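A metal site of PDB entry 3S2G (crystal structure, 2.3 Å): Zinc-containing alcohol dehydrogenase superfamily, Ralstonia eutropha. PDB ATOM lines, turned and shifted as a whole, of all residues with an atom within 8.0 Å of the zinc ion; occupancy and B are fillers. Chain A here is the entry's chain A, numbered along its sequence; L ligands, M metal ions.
A ring nitrogen (NE2) of His 63 sits close to an oxygen (O2) of the ligand (2.7 Å). The side-chain sulfur (SG) of Cys 150 sits close to an oxygen (O2) of the ligand, at 3.1 Å. An oxygen (O2) of the ligand sits close to the side-chain sulfur (SG) of Cys 40 (3.5 Å). OG1 of Thr 42 is in hydrogen-bond range of O2 of the ligand, 2.7 Å away.
The side-chain carboxylate (OE1) of Glu 64 lies within salt-bridge range of the guanidinium group (NH2) of Arg 333 (3.4 Å). O of Glu 64 lies within hydrogen-bond range of N of Gly 38. ND1 of His 63 lies close to OD1 of Asp 43. The backbone carbonyl oxygen (O) of Cys 150 lies within hydrogen-bond range of the side-chain hydroxyl (OG1) of Thr 154 (2.8 Å). The backbone NH (N) of Thr 42 lies close to the side-chain sulfur (SG) of Cys 40. The backbone NH (N) of Cys 40 is in hydrogen-bond range of the side-chain carboxylate (OD2) of Asp 43 (3.1 Å).
The zinc ion is bound by the side-chain carboxylate of Glu 64, a ring nitrogen (NE2) of His 63, the side-chain sulfur of Cys 150 and the side-chain sulfur of Cys 40.
Four residues have an atom within 4 Å of the zinc ion: Cys 40, His 63, Glu 64 and Cys 150. The nearest printed residue that does not touch the zinc ion is Arg 333 (4.1 Å).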
ATOM      1  N   GLY A  38       1.453  27.854  -3.665  1.00  0.00           N
ATOM      2  CA  GLY A  38       1.109  27.085  -2.484  1.00  0.00           C
ATOM      3  C   GLY A  38       2.275  26.814  -1.547  1.00  0.00           C
ATOM      4  O   GLY A  38       3.422  26.674  -1.987  1.00  0.00           O
ATOM      5  N   VAL A  39       1.974  26.755  -0.259  1.00  0.00           N
ATOM      6  CA  VAL A  39       2.977  26.483   0.773  1.00  0.00           C
ATOM      7  C   VAL A  39       2.585  25.237   1.558  1.00  0.00           C
ATOM      8  O   VAL A  39       1.419  25.062   1.915  1.00  0.00           O
ATOM      9  CB  VAL A  39       3.102  27.662   1.750  1.00  0.00           C
ATOM     10  CG1 VAL A  39       4.147  27.358   2.817  1.00  0.00           C
ATOM     11  CG2 VAL A  39       3.438  28.945   1.007  1.00  0.00           C
ATOM     12  N   CYS A  40       3.556  24.367   1.822  1.00  0.00           N
ATOM     13  CA  CYS A  40       3.305  23.155   2.586  1.00  0.00           C
ATOM     14  C   CYS A  40       4.531  22.800   3.444  1.00  0.00           C
ATOM     15  O   CYS A  40       5.561  23.458   3.368  1.00  0.00           O
ATOM     16  CB  CYS A  40       2.988  21.990   1.650  1.00  0.00           C
ATOM     17  SG  CYS A  40       4.439  21.061   1.144  1.00  0.00           S
ATOM     18  N   HIS A  41       4.395  21.749   4.242  1.00  0.00           N
ATOM     19  CA  HIS A  41       5.447  21.330   5.165  1.00  0.00           C
ATOM     20  C   HIS A  41       6.750  20.894   4.475  1.00  0.00           C
ATOM     21  O   HIS A  41       7.810  20.918   5.095  1.00  0.00           O
ATOM     22  CB  HIS A  41       4.946  20.223   6.098  1.00  0.00           C
ATOM     23  CG  HIS A  41       4.205  20.743   7.292  1.00  0.00           C
ATOM     24  ND1 HIS A  41       4.826  21.055   8.483  1.00  0.00           N
ATOM     25  CD2 HIS A  41       2.891  21.008   7.478  1.00  0.00           C
ATOM     26  CE1 HIS A  41       3.922  21.496   9.352  1.00  0.00           C
ATOM     27  NE2 HIS A  41       2.740  21.469   8.765  1.00  0.00           N
ATOM     28  N   THR A  42       6.664  20.501   3.212  1.00  0.00           N
ATOM     29  CA  THR A  42       7.848  20.136   2.449  1.00  0.00           C
ATOM     30  C   THR A  42       8.771  21.344   2.322  1.00  0.00           C
ATOM     31  O   THR A  42       9.995  21.208   2.316  1.00  0.00           O
ATOM     32  CB  THR A  42       7.488  19.620   1.043  1.00  0.00           C
ATOM     33  OG1 THR A  42       6.854  18.346   1.156  1.00  0.00           O
ATOM     34  CG2 THR A  42       8.738  19.488   0.182  1.00  0.00           C
ATOM     35  N   ASP A  43       8.171  22.523   2.239  1.00  0.00           N
ATOM     36  CA  ASP A  43       8.922  23.774   2.151  1.00  0.00           C
ATOM     37  C   ASP A  43       9.721  24.019   3.434  1.00  0.00           C
ATOM     38  O   ASP A  43      10.800  24.594   3.399  1.00  0.00           O
ATOM     39  CB  ASP A  43       7.997  24.955   1.864  1.00  0.00           C
ATOM     40  CG  ASP A  43       7.255  24.794   0.548  1.00  0.00           C
ATOM     41  OD1 ASP A  43       7.820  24.161  -0.376  1.00  0.00           O
ATOM     42  OD2 ASP A  43       6.127  25.313   0.429  1.00  0.00           O
ATOM     43  N   GLY A  62       9.254  26.385  -3.173  1.00  0.00           N
ATOM     44  CA  GLY A  62       7.977  26.480  -3.865  1.00  0.00           C
ATOM     45  C   GLY A  62       7.812  25.482  -4.993  1.00  0.00           C
ATOM     46  O   GLY A  62       8.403  25.636  -6.069  1.00  0.00           O
ATOM     47  N   HIS A  63       6.986  24.471  -4.765  1.00  0.00           N
ATOM     48  CA  HIS A  63       6.678  23.474  -5.775  1.00  0.00           C
ATOM     49  C   HIS A  63       5.170  23.432  -6.042  1.00  0.00           C
ATOM     50  O   HIS A  63       4.647  22.454  -6.579  1.00  0.00           O
ATOM     51  CB  HIS A  63       7.185  22.092  -5.364  1.00  0.00           C
ATOM     52  CG  HIS A  63       6.699  21.648  -4.014  1.00  0.00           C
ATOM     53  ND1 HIS A  63       7.309  22.041  -2.839  1.00  0.00           N
ATOM     54  CD2 HIS A  63       5.666  20.864  -3.654  1.00  0.00           C
ATOM     55  CE1 HIS A  63       6.664  21.508  -1.813  1.00  0.00           C
ATOM     56  NE2 HIS A  63       5.662  20.787  -2.284  1.00  0.00           N
ATOM     57  N   GLU A  64       4.489  24.510  -5.665  1.00  0.00           N
ATOM     58  CA  GLU A  64       3.059  24.645  -5.916  1.00  0.00           C
ATOM     59  C   GLU A  64       2.763  25.968  -6.598  1.00  0.00           C
ATOM     60  O   GLU A  64       1.727  26.587  -6.342  1.00  0.00           O
ATOM     61  CB  GLU A  64       2.272  24.538  -4.618  1.00  0.00           C
ATOM     62  CG  GLU A  64       2.556  23.306  -3.790  1.00  0.00           C
ATOM     63  CD  GLU A  64       1.758  23.280  -2.507  1.00  0.00           C
ATOM     64  OE1 GLU A  64       0.677  23.916  -2.471  1.00  0.00           O
ATOM     65  OE2 GLU A  64       2.193  22.645  -1.524  1.00  0.00           O
ATOM     66  N   TRP A  89       6.239  19.483  -7.922  1.00  0.00           N
ATOM     67  CA  TRP A  89       7.411  18.841  -7.324  1.00  0.00           C
ATOM     68  C   TRP A  89       8.353  18.230  -8.350  1.00  0.00           C
ATOM     69  O   TRP A  89       9.561  18.455  -8.310  1.00  0.00           O
ATOM     70  CB  TRP A  89       6.952  17.758  -6.340  1.00  0.00           C
ATOM     71  CG  TRP A  89       8.076  17.004  -5.691  1.00  0.00           C
ATOM     72  CD1 TRP A  89       8.414  15.687  -5.891  1.00  0.00           C
ATOM     73  CD2 TRP A  89       9.003  17.501  -4.716  1.00  0.00           C
ATOM     74  NE1 TRP A  89       9.494  15.360  -5.104  1.00  0.00           N
ATOM     75  CE2 TRP A  89       9.873  16.446  -4.376  1.00  0.00           C
ATOM     76  CE3 TRP A  89       9.180  18.749  -4.106  1.00  0.00           C
ATOM     77  CZ2 TRP A  89      10.907  16.599  -3.450  1.00  0.00           C
ATOM     78  CZ3 TRP A  89      10.208  18.898  -3.188  1.00  0.00           C
ATOM     79  CH2 TRP A  89      11.057  17.821  -2.875  1.00  0.00           C
ATOM     80  N   TYR A 122       8.509  30.428  -5.193  1.00  0.00           N
ATOM     81  CA  TYR A 122       8.512  31.493  -4.199  1.00  0.00           C
ATOM     82  C   TYR A 122       9.045  32.791  -4.793  1.00  0.00           C
ATOM     83  O   TYR A 122       9.724  33.569  -4.124  1.00  0.00           O
ATOM     84  CB  TYR A 122       9.337  31.099  -2.961  1.00  0.00           C
ATOM     85  CG  TYR A 122       8.598  30.241  -1.951  1.00  0.00           C
ATOM     86  CD1 TYR A 122       8.955  30.257  -0.606  1.00  0.00           C
ATOM     87  CD2 TYR A 122       7.536  29.419  -2.338  1.00  0.00           C
ATOM     88  CE1 TYR A 122       8.295  29.474   0.316  1.00  0.00           C
ATOM     89  CE2 TYR A 122       6.869  28.635  -1.409  1.00  0.00           C
ATOM     90  CZ  TYR A 122       7.256  28.671  -0.085  1.00  0.00           C
ATOM     91  OH  TYR A 122       6.602  27.892   0.845  1.00  0.00           O
ATOM     92  N   ALA A 146      -3.779  25.894  -6.711  1.00  0.00           N
ATOM     93  CA  ALA A 146      -2.379  25.710  -6.328  1.00  0.00           C
ATOM     94  C   ALA A 146      -2.102  24.442  -5.504  1.00  0.00           C
ATOM     95  O   ALA A 146      -1.204  23.680  -5.827  1.00  0.00           O
ATOM     96  CB  ALA A 146      -1.845  26.958  -5.612  1.00  0.00           C
ATOM     97  N   PRO A 147      -2.868  24.227  -4.421  1.00  0.00           N
ATOM     98  CA  PRO A 147      -2.637  23.080  -3.534  1.00  0.00           C
ATOM     99  C   PRO A 147      -2.836  21.725  -4.214  1.00  0.00           C
ATOM    100  O   PRO A 147      -2.334  20.714  -3.713  1.00  0.00           O
ATOM    101  CB  PRO A 147      -3.685  23.263  -2.436  1.00  0.00           C
ATOM    102  CG  PRO A 147      -4.006  24.720  -2.456  1.00  0.00           C
ATOM    103  CD  PRO A 147      -3.919  25.117  -3.895  1.00  0.00           C
ATOM    104  N   LEU A 149      -1.558  20.809  -6.908  1.00  0.00           N
ATOM    105  CA  LEU A 149      -0.268  20.430  -7.462  1.00  0.00           C
ATOM    106  C   LEU A 149       0.515  19.519  -6.523  1.00  0.00           C
ATOM    107  O   LEU A 149       1.433  18.828  -6.951  1.00  0.00           O
ATOM    108  CB  LEU A 149       0.579  21.670  -7.762  1.00  0.00           C
ATOM    109  CG  LEU A 149       0.140  22.564  -8.909  1.00  0.00           C
ATOM    110  CD1 LEU A 149       1.088  23.750  -9.032  1.00  0.00           C
ATOM    111  CD2 LEU A 149       0.095  21.768 -10.205  1.00  0.00           C
ATOM    112  N   CYS A 150       0.150  19.541  -5.248  1.00  0.00           N
ATOM    113  CA  CYS A 150       0.872  18.753  -4.262  1.00  0.00           C
ATOM    114  C   CYS A 150      -0.074  17.907  -3.419  1.00  0.00           C
ATOM    115  O   CYS A 150      -0.102  16.688  -3.543  1.00  0.00           O
ATOM    116  CB  CYS A 150       1.693  19.667  -3.347  1.00  0.00           C
ATOM    117  SG  CYS A 150       2.413  18.816  -1.941  1.00  0.00           S
ATOM    118  N   ALA A 151      -0.831  18.563  -2.540  1.00  0.00           N
ATOM    119  CA  ALA A 151      -1.795  17.872  -1.699  1.00  0.00           C
ATOM    120  C   ALA A 151      -2.782  17.073  -2.547  1.00  0.00           C
ATOM    121  O   ALA A 151      -3.084  15.921  -2.228  1.00  0.00           O
ATOM    122  CB  ALA A 151      -2.529  18.855  -0.817  1.00  0.00           C
ATOM    123  N   GLY A 152      -3.267  17.686  -3.617  1.00  0.00           N
ATOM    124  CA  GLY A 152      -4.250  17.061  -4.483  1.00  0.00           C
ATOM    125  C   GLY A 152      -3.790  15.740  -5.087  1.00  0.00           C
ATOM    126  O   GLY A 152      -4.330  14.684  -4.782  1.00  0.00           O
ATOM    127  N   THR A 154      -1.180  14.033  -4.517  1.00  0.00           N
ATOM    128  CA  THR A 154      -0.671  13.129  -3.492  1.00  0.00           C
ATOM    129  C   THR A 154      -1.747  12.197  -2.956  1.00  0.00           C
ATOM    130  O   THR A 154      -1.579  10.978  -2.966  1.00  0.00           O
ATOM    131  CB  THR A 154      -0.043  13.899  -2.320  1.00  0.00           C
ATOM    132  OG1 THR A 154       1.240  14.400  -2.724  1.00  0.00           O
ATOM    133  CG2 THR A 154       0.128  12.999  -1.115  1.00  0.00           C
ATOM    134  N   LEU A 178      -3.741  17.500   3.995  1.00  0.00           N
ATOM    135  CA  LEU A 178      -3.919  16.450   3.000  1.00  0.00           C
ATOM    136  C   LEU A 178      -5.280  15.766   3.182  1.00  0.00           C
ATOM    137  O   LEU A 178      -6.030  15.597   2.223  1.00  0.00           O
ATOM    138  CB  LEU A 178      -2.813  15.398   3.116  1.00  0.00           C
ATOM    139  CG  LEU A 178      -1.371  15.841   2.845  1.00  0.00           C
ATOM    140  CD1 LEU A 178      -0.441  14.648   2.869  1.00  0.00           C
ATOM    141  CD2 LEU A 178      -1.287  16.545   1.508  1.00  0.00           C
ATOM    142  N   ILE A 287       3.675   9.370  -2.611  1.00  0.00           N
ATOM    143  CA  ILE A 287       3.648  10.828  -2.487  1.00  0.00           C
ATOM    144  C   ILE A 287       3.667  11.455  -3.871  1.00  0.00           C
ATOM    145  O   ILE A 287       4.242  10.889  -4.809  1.00  0.00           O
ATOM    146  CB  ILE A 287       4.825  11.358  -1.626  1.00  0.00           C
ATOM    147  CG1 ILE A 287       4.663  12.854  -1.367  1.00  0.00           C
ATOM    148  CG2 ILE A 287       6.168  11.062  -2.291  1.00  0.00           C
ATOM    149  CD1 ILE A 287       5.602  13.408  -0.334  1.00  0.00           C
ATOM    150  N   VAL A 288       3.041  12.627  -4.012  1.00  0.00           N
ATOM    151  CA  VAL A 288       2.768  13.230  -5.323  1.00  0.00           C
ATOM    152  C   VAL A 288       2.344  12.182  -6.350  1.00  0.00           C
ATOM    153  O   VAL A 288       1.747  11.164  -5.990  1.00  0.00           O
ATOM    154  CB  VAL A 288       3.960  14.068  -5.854  1.00  0.00           C
ATOM    155  CG1 VAL A 288       4.233  15.246  -4.930  1.00  0.00           C
ATOM    156  CG2 VAL A 288       5.205  13.219  -6.034  1.00  0.00           C
ATOM    157  N   ARG A 333      -4.861  24.834   3.792  1.00  0.00           N
ATOM    158  CA  ARG A 333      -3.588  25.158   3.163  1.00  0.00           C
ATOM    159  C   ARG A 333      -3.393  26.658   3.000  1.00  0.00           C
ATOM    160  O   ARG A 333      -4.355  27.395   2.778  1.00  0.00           O
ATOM    161  CB  ARG A 333      -3.469  24.486   1.795  1.00  0.00           C
ATOM    162  CG  ARG A 333      -3.019  23.030   1.832  1.00  0.00           C
ATOM    163  CD  ARG A 333      -1.547  22.916   2.191  1.00  0.00           C
ATOM    164  NE  ARG A 333      -1.085  21.528   2.129  1.00  0.00           N
ATOM    165  CZ  ARG A 333      -0.432  21.004   1.093  1.00  0.00           C
ATOM    166  NH1 ARG A 333      -0.049  19.727   1.127  1.00  0.00           N
ATOM    167  NH2 ARG A 333      -0.166  21.733   0.025  1.00  0.00           N
HETATM  168  C1  LIG L   1       5.549  17.556  -2.091  1.00  0.00           C
HETATM  169  C2  LIG L   1       6.619  16.535  -1.959  1.00  0.00           C
HETATM  170  O1  LIG L   1       7.518  16.490  -0.952  1.00  0.00           O
HETATM  171  C3  LIG L   1       8.356  15.441  -1.114  1.00  0.00           C
HETATM  172  C4  LIG L   1       7.974  14.776  -2.264  1.00  0.00           C
HETATM  173  C5  LIG L   1       6.883  15.461  -2.797  1.00  0.00           C
HETATM  174  O2  LIG L   1       5.359  18.419  -1.033  1.00  0.00           O
HETATM  175 ZN    ZN M   1       3.613  20.927  -1.250  1.00  0.00          ZN
